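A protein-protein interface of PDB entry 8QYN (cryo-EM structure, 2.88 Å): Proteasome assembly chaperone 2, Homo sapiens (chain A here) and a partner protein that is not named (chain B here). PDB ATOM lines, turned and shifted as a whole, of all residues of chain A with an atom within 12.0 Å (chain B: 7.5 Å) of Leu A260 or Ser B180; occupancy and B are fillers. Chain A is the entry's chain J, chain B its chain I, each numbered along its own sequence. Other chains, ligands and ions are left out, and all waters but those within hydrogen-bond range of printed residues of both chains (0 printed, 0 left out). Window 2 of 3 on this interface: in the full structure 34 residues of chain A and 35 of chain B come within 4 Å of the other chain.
Leu A260 touches one residue of chain B.
Of chain A, only Leu A260 (3.5 Å) comes within 4 Å of Ser B180.
Glu B179 touches just these residues of chain A: Ser A258 (3.7 Å) and Gly A259 (3.1 Å).
Ser B183 touches none of the printed residues of chain A.
Of the printed residues of chain B, Gly A259 touches Thr B177, Ser B178 and Glu B179.
Printed residues of chain B within 4 Å of Ser A258: Tyr B175 (3.5 Å), Thr B177 (3.2 Å), Glu B179 (3.7 Å) and Thr B181 (3.9 Å).
Of the printed residues of chain B, Leu A254 touches Thr B177 (3.9 Å) and Ser B178 (3.9 Å).
Pro A261 touches none of the printed residues of chain B.
Arg A253 touches none of the printed residues of chain B.
The nearest residue of chain B that does not touch Leu A260 is Ser B178 (5.3 Å).
C of Thr B177 touches CD1 of Leu A254 (3.9 Å).
Ser B178 touches Leu A254.
OG of Ser A258 touches O of Tyr B175, 3.5 Å away.
O of Thr B177 touches CA of Ser A258, at 3.2 Å.
Glu B179 touches Ser A258.
OG1 of Thr B181 touches OG of Ser A258, at 3.9 Å.
N of Gly A259 touches O of Thr B177, 3.8 Å away.
Ser B180 touches Leu A260 (CB to O, 3.5 Å).
N of Gly A259 sits at hydrogen-bond distance from O of Ser B178, 3.3 Å away.
The backbone carbonyl oxygen (O) of Glu B179 lies within hydrogen-bond range of the backbone NH (N) of Gly A259 (3.1 Å).
Printed residues of chain A that touch a printed residue of chain B: Leu A254, Ser A258, Gly A259 and Leu A260.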
ATOM      1  N   ARG A 253     -17.276  -3.922 -13.331  1.00  0.00           N
ATOM      2  CA  ARG A 253     -18.209  -4.684 -12.518  1.00  0.00           C
ATOM      3  C   ARG A 253     -19.286  -5.273 -13.413  1.00  0.00           C
ATOM      4  O   ARG A 253     -19.569  -4.750 -14.493  1.00  0.00           O
ATOM      5  CB  ARG A 253     -18.838  -3.823 -11.414  1.00  0.00           C
ATOM      6  CG  ARG A 253     -19.762  -2.733 -11.907  1.00  0.00           C
ATOM      7  CD  ARG A 253     -20.437  -2.036 -10.740  1.00  0.00           C
ATOM      8  NE  ARG A 253     -21.618  -1.292 -11.158  1.00  0.00           N
ATOM      9  CZ  ARG A 253     -22.863  -1.733 -11.038  1.00  0.00           C
ATOM     10  NH1 ARG A 253     -23.129  -2.916 -10.509  1.00  0.00           N
ATOM     11  NH2 ARG A 253     -23.866  -0.970 -11.461  1.00  0.00           N
ATOM     12  N   LEU A 254     -19.885  -6.370 -12.948  1.00  0.00           N
ATOM     13  CA  LEU A 254     -20.869  -7.126 -13.724  1.00  0.00           C
ATOM     14  C   LEU A 254     -20.294  -7.563 -15.068  1.00  0.00           C
ATOM     15  O   LEU A 254     -20.963  -7.500 -16.100  1.00  0.00           O
ATOM     16  CB  LEU A 254     -22.157  -6.324 -13.921  1.00  0.00           C
ATOM     17  CG  LEU A 254     -22.959  -6.010 -12.661  1.00  0.00           C
ATOM     18  CD1 LEU A 254     -24.103  -5.077 -12.986  1.00  0.00           C
ATOM     19  CD2 LEU A 254     -23.477  -7.285 -12.032  1.00  0.00           C
ATOM     20  N   PHE A 256     -19.489 -10.578 -15.972  1.00  0.00           N
ATOM     21  CA  PHE A 256     -20.044 -11.859 -16.384  1.00  0.00           C
ATOM     22  C   PHE A 256     -21.550 -11.813 -16.618  1.00  0.00           C
ATOM     23  O   PHE A 256     -22.135 -12.835 -16.985  1.00  0.00           O
ATOM     24  CB  PHE A 256     -19.721 -12.929 -15.341  1.00  0.00           C
ATOM     25  CG  PHE A 256     -18.481 -13.720 -15.645  1.00  0.00           C
ATOM     26  CD1 PHE A 256     -18.498 -14.728 -16.590  1.00  0.00           C
ATOM     27  CD2 PHE A 256     -17.300 -13.464 -14.972  1.00  0.00           C
ATOM     28  CE1 PHE A 256     -17.360 -15.457 -16.865  1.00  0.00           C
ATOM     29  CE2 PHE A 256     -16.161 -14.192 -15.244  1.00  0.00           C
ATOM     30  CZ  PHE A 256     -16.191 -15.188 -16.190  1.00  0.00           C
ATOM     31  N   GLY A 257     -22.191 -10.663 -16.416  1.00  0.00           N
ATOM     32  CA  GLY A 257     -23.613 -10.542 -16.672  1.00  0.00           C
ATOM     33  C   GLY A 257     -24.443 -10.221 -15.447  1.00  0.00           C
ATOM     34  O   GLY A 257     -23.938  -9.647 -14.480  1.00  0.00           O
ATOM     35  N   SER A 258     -25.720 -10.590 -15.476  1.00  0.00           N
ATOM     36  CA  SER A 258     -26.649 -10.285 -14.399  1.00  0.00           C
ATOM     37  C   SER A 258     -26.674 -11.427 -13.383  1.00  0.00           C
ATOM     38  O   SER A 258     -25.839 -12.333 -13.410  1.00  0.00           O
ATOM     39  CB  SER A 258     -28.035 -10.004 -14.969  1.00  0.00           C
ATOM     40  OG  SER A 258     -27.963  -9.098 -16.053  1.00  0.00           O
ATOM     41  N   GLY A 259     -27.646 -11.391 -12.468  1.00  0.00           N
ATOM     42  CA  GLY A 259     -27.738 -12.369 -11.405  1.00  0.00           C
ATOM     43  C   GLY A 259     -28.456 -13.644 -11.817  1.00  0.00           C
ATOM     44  O   GLY A 259     -28.916 -13.807 -12.945  1.00  0.00           O
ATOM     45  N   LEU A 260     -28.545 -14.566 -10.856  1.00  0.00           N
ATOM     46  CA  LEU A 260     -29.134 -15.884 -11.052  1.00  0.00           C
ATOM     47  C   LEU A 260     -30.658 -15.804 -11.082  1.00  0.00           C
ATOM     48  O   LEU A 260     -31.254 -15.004 -10.359  1.00  0.00           O
ATOM     49  CB  LEU A 260     -28.704 -16.829  -9.934  1.00  0.00           C
ATOM     50  CG  LEU A 260     -27.448 -17.670 -10.120  1.00  0.00           C
ATOM     51  CD1 LEU A 260     -26.922 -18.099  -8.771  1.00  0.00           C
ATOM     52  CD2 LEU A 260     -27.762 -18.881 -10.969  1.00  0.00           C
ATOM     53  N   PRO A 261     -31.311 -16.629 -11.902  1.00  0.00           N
ATOM     54  CA  PRO A 261     -32.755 -16.793 -11.770  1.00  0.00           C
ATOM     55  C   PRO A 261     -33.094 -17.490 -10.468  1.00  0.00           C
ATOM     56  O   PRO A 261     -32.277 -18.253  -9.924  1.00  0.00           O
ATOM     57  CB  PRO A 261     -33.127 -17.657 -12.988  1.00  0.00           C
ATOM     58  CG  PRO A 261     -31.864 -18.321 -13.386  1.00  0.00           C
ATOM     59  CD  PRO A 261     -30.769 -17.368 -13.053  1.00  0.00           C
ATOM     60  N   PRO A 262     -34.287 -17.259  -9.922  1.00  0.00           N
ATOM     61  CA  PRO A 262     -34.577 -17.717  -8.555  1.00  0.00           C
ATOM     62  C   PRO A 262     -34.664 -19.227  -8.373  1.00  0.00           C
ATOM     63  O   PRO A 262     -34.019 -19.778  -7.476  1.00  0.00           O
ATOM     64  CB  PRO A 262     -35.924 -17.051  -8.249  1.00  0.00           C
ATOM     65  CG  PRO A 262     -36.542 -16.818  -9.576  1.00  0.00           C
ATOM     66  CD  PRO A 262     -35.414 -16.518 -10.509  1.00  0.00           C
ATOM     67  N   ALA A 263     -35.446 -19.912  -9.204  1.00  0.00           N
ATOM     68  CA  ALA A 263     -35.857 -21.288  -8.932  1.00  0.00           C
ATOM     69  C   ALA A 263     -35.000 -22.315  -9.656  1.00  0.00           C
ATOM     70  O   ALA A 263     -35.504 -23.352 -10.093  1.00  0.00           O
ATOM     71  CB  ALA A 263     -37.326 -21.477  -9.292  1.00  0.00           C
ATOM     72  N   LEU A 264     -33.700 -22.062  -9.796  1.00  0.00           N
ATOM     73  CA  LEU A 264     -32.799 -22.986 -10.474  1.00  0.00           C
ATOM     74  C   LEU A 264     -31.967 -23.815  -9.504  1.00  0.00           C
ATOM     75  O   LEU A 264     -31.866 -25.034  -9.662  1.00  0.00           O
ATOM     76  CB  LEU A 264     -31.877 -22.215 -11.422  1.00  0.00           C
ATOM     77  CG  LEU A 264     -31.409 -22.971 -12.661  1.00  0.00           C
ATOM     78  CD1 LEU A 264     -32.574 -23.241 -13.578  1.00  0.00           C
ATOM     79  CD2 LEU A 264     -30.336 -22.184 -13.383  1.00  0.00           C
ATOM     80  N   PHE A 265     -31.369 -23.176  -8.505  1.00  0.00           N
ATOM     81  CA  PHE A 265     -30.521 -23.872  -7.544  1.00  0.00           C
ATOM     82  C   PHE A 265     -31.246 -24.086  -6.221  1.00  0.00           C
ATOM     83  O   PHE A 265     -32.469 -24.207  -6.184  1.00  0.00           O
ATOM     84  CB  PHE A 265     -29.228 -23.091  -7.310  1.00  0.00           C
ATOM     85  CG  PHE A 265     -28.198 -23.298  -8.375  1.00  0.00           C
ATOM     86  CD1 PHE A 265     -28.239 -22.565  -9.545  1.00  0.00           C
ATOM     87  CD2 PHE A 265     -27.190 -24.226  -8.211  1.00  0.00           C
ATOM     88  CE1 PHE A 265     -27.296 -22.755 -10.530  1.00  0.00           C
ATOM     89  CE2 PHE A 265     -26.244 -24.418  -9.193  1.00  0.00           C
ATOM     90  CZ  PHE A 265     -26.299 -23.681 -10.354  1.00  0.00           C
ATOM     91  N   TYR B 175     -30.270  -5.324 -20.246  1.00  0.00           N
ATOM     92  CA  TYR B 175     -29.952  -4.454 -19.123  1.00  0.00           C
ATOM     93  C   TYR B 175     -29.030  -5.174 -18.148  1.00  0.00           C
ATOM     94  O   TYR B 175     -29.293  -6.317 -17.762  1.00  0.00           O
ATOM     95  CB  TYR B 175     -31.236  -4.020 -18.421  1.00  0.00           C
ATOM     96  CG  TYR B 175     -31.078  -2.811 -17.536  1.00  0.00           C
ATOM     97  CD1 TYR B 175     -30.731  -1.583 -18.065  1.00  0.00           C
ATOM     98  CD2 TYR B 175     -31.282  -2.899 -16.170  1.00  0.00           C
ATOM     99  CE1 TYR B 175     -30.588  -0.478 -17.261  1.00  0.00           C
ATOM    100  CE2 TYR B 175     -31.141  -1.800 -15.359  1.00  0.00           C
ATOM    101  CZ  TYR B 175     -30.794  -0.593 -15.909  1.00  0.00           C
ATOM    102  OH  TYR B 175     -30.652   0.507 -15.101  1.00  0.00           O
ATOM    103  N   THR B 177     -27.725  -5.607 -14.547  1.00  0.00           N
ATOM    104  CA  THR B 177     -28.070  -5.324 -13.164  1.00  0.00           C
ATOM    105  C   THR B 177     -27.632  -6.493 -12.296  1.00  0.00           C
ATOM    106  O   THR B 177     -27.511  -7.623 -12.771  1.00  0.00           O
ATOM    107  CB  THR B 177     -29.570  -5.069 -12.993  1.00  0.00           C
ATOM    108  OG1 THR B 177     -29.866  -4.862 -11.607  1.00  0.00           O
ATOM    109  CG2 THR B 177     -30.371  -6.251 -13.503  1.00  0.00           C
ATOM    110  N   SER B 178     -27.390  -6.207 -11.014  1.00  0.00           N
ATOM    111  CA  SER B 178     -26.917  -7.243 -10.104  1.00  0.00           C
ATOM    112  C   SER B 178     -27.980  -8.309  -9.870  1.00  0.00           C
ATOM    113  O   SER B 178     -27.663  -9.499  -9.779  1.00  0.00           O
ATOM    114  CB  SER B 178     -26.480  -6.621  -8.779  1.00  0.00           C
ATOM    115  OG  SER B 178     -27.595  -6.145  -8.050  1.00  0.00           O
ATOM    116  N   GLU B 179     -29.240  -7.905  -9.766  1.00  0.00           N
ATOM    117  CA  GLU B 179     -30.331  -8.846  -9.551  1.00  0.00           C
ATOM    118  C   GLU B 179     -30.642  -9.574 -10.857  1.00  0.00           C
ATOM    119  O   GLU B 179     -29.979  -9.391 -11.881  1.00  0.00           O
ATOM    120  CB  GLU B 179     -31.555  -8.119  -9.007  1.00  0.00           C
ATOM    121  CG  GLU B 179     -31.372  -7.546  -7.622  1.00  0.00           C
ATOM    122  CD  GLU B 179     -32.232  -6.324  -7.390  1.00  0.00           C
ATOM    123  OE1 GLU B 179     -32.530  -5.618  -8.375  1.00  0.00           O
ATOM    124  OE2 GLU B 179     -32.613  -6.072  -6.229  1.00  0.00           O
ATOM    125  N   SER B 180     -31.668 -10.418 -10.832  1.00  0.00           N
ATOM    126  CA  SER B 180     -32.098 -11.111 -12.033  1.00  0.00           C
ATOM    127  C   SER B 180     -32.838 -10.157 -12.961  1.00  0.00           C
ATOM    128  O   SER B 180     -33.427  -9.165 -12.526  1.00  0.00           O
ATOM    129  CB  SER B 180     -32.996 -12.295 -11.680  1.00  0.00           C
ATOM    130  OG  SER B 180     -33.937 -11.940 -10.684  1.00  0.00           O
ATOM    131  N   THR B 181     -32.794 -10.464 -14.259  1.00  0.00           N
ATOM    132  CA  THR B 181     -33.478  -9.627 -15.240  1.00  0.00           C
ATOM    133  C   THR B 181     -34.988  -9.661 -15.042  1.00  0.00           C
ATOM    134  O   THR B 181     -35.658  -8.626 -15.142  1.00  0.00           O
ATOM    135  CB  THR B 181     -33.118 -10.075 -16.656  1.00  0.00           C
ATOM    136  OG1 THR B 181     -31.705  -9.960 -16.852  1.00  0.00           O
ATOM    137  CG2 THR B 181     -33.828  -9.214 -17.677  1.00  0.00           C
ATOM    138  N   GLY B 182     -35.542 -10.836 -14.754  1.00  0.00           N
ATOM    139  CA  GLY B 182     -36.980 -10.981 -14.619  1.00  0.00           C
ATOM    140  C   GLY B 182     -37.583 -10.267 -13.429  1.00  0.00           C
ATOM    141  O   GLY B 182     -38.807 -10.102 -13.387  1.00  0.00           O
ATOM    142  N   SER B 183     -36.765  -9.844 -12.467  1.00  0.00           N
ATOM    143  CA  SER B 183     -37.265  -9.158 -11.284  1.00  0.00           C
ATOM    144  C   SER B 183     -37.539  -7.678 -11.517  1.00  0.00           C
ATOM    145  O   SER B 183     -38.194  -7.050 -10.679  1.00  0.00           O
ATOM    146  CB  SER B 183     -36.272  -9.316 -10.131  1.00  0.00           C
ATOM    147  OG  SER B 183     -36.616  -8.478  -9.045  1.00  0.00           O
ATOM    148  N   LEU B 184     -37.057  -7.109 -12.618  1.00  0.00           N
ATOM    149  CA  LEU B 184     -37.251  -5.695 -12.896  1.00  0.00           C
ATOM    150  C   LEU B 184     -38.694  -5.413 -13.310  1.00  0.00           C
ATOM    151  O   LEU B 184     -39.336  -6.245 -13.956  1.00  0.00           O
ATOM    152  CB  LEU B 184     -36.303  -5.236 -13.996  1.00  0.00           C
ATOM    153  CG  LEU B 184     -34.810  -5.404 -13.716  1.00  0.00           C
ATOM    154  CD1 LEU B 184     -34.042  -5.564 -15.012  1.00  0.00           C
ATOM    155  CD2 LEU B 184     -34.283  -4.222 -12.926  1.00  0.00           C
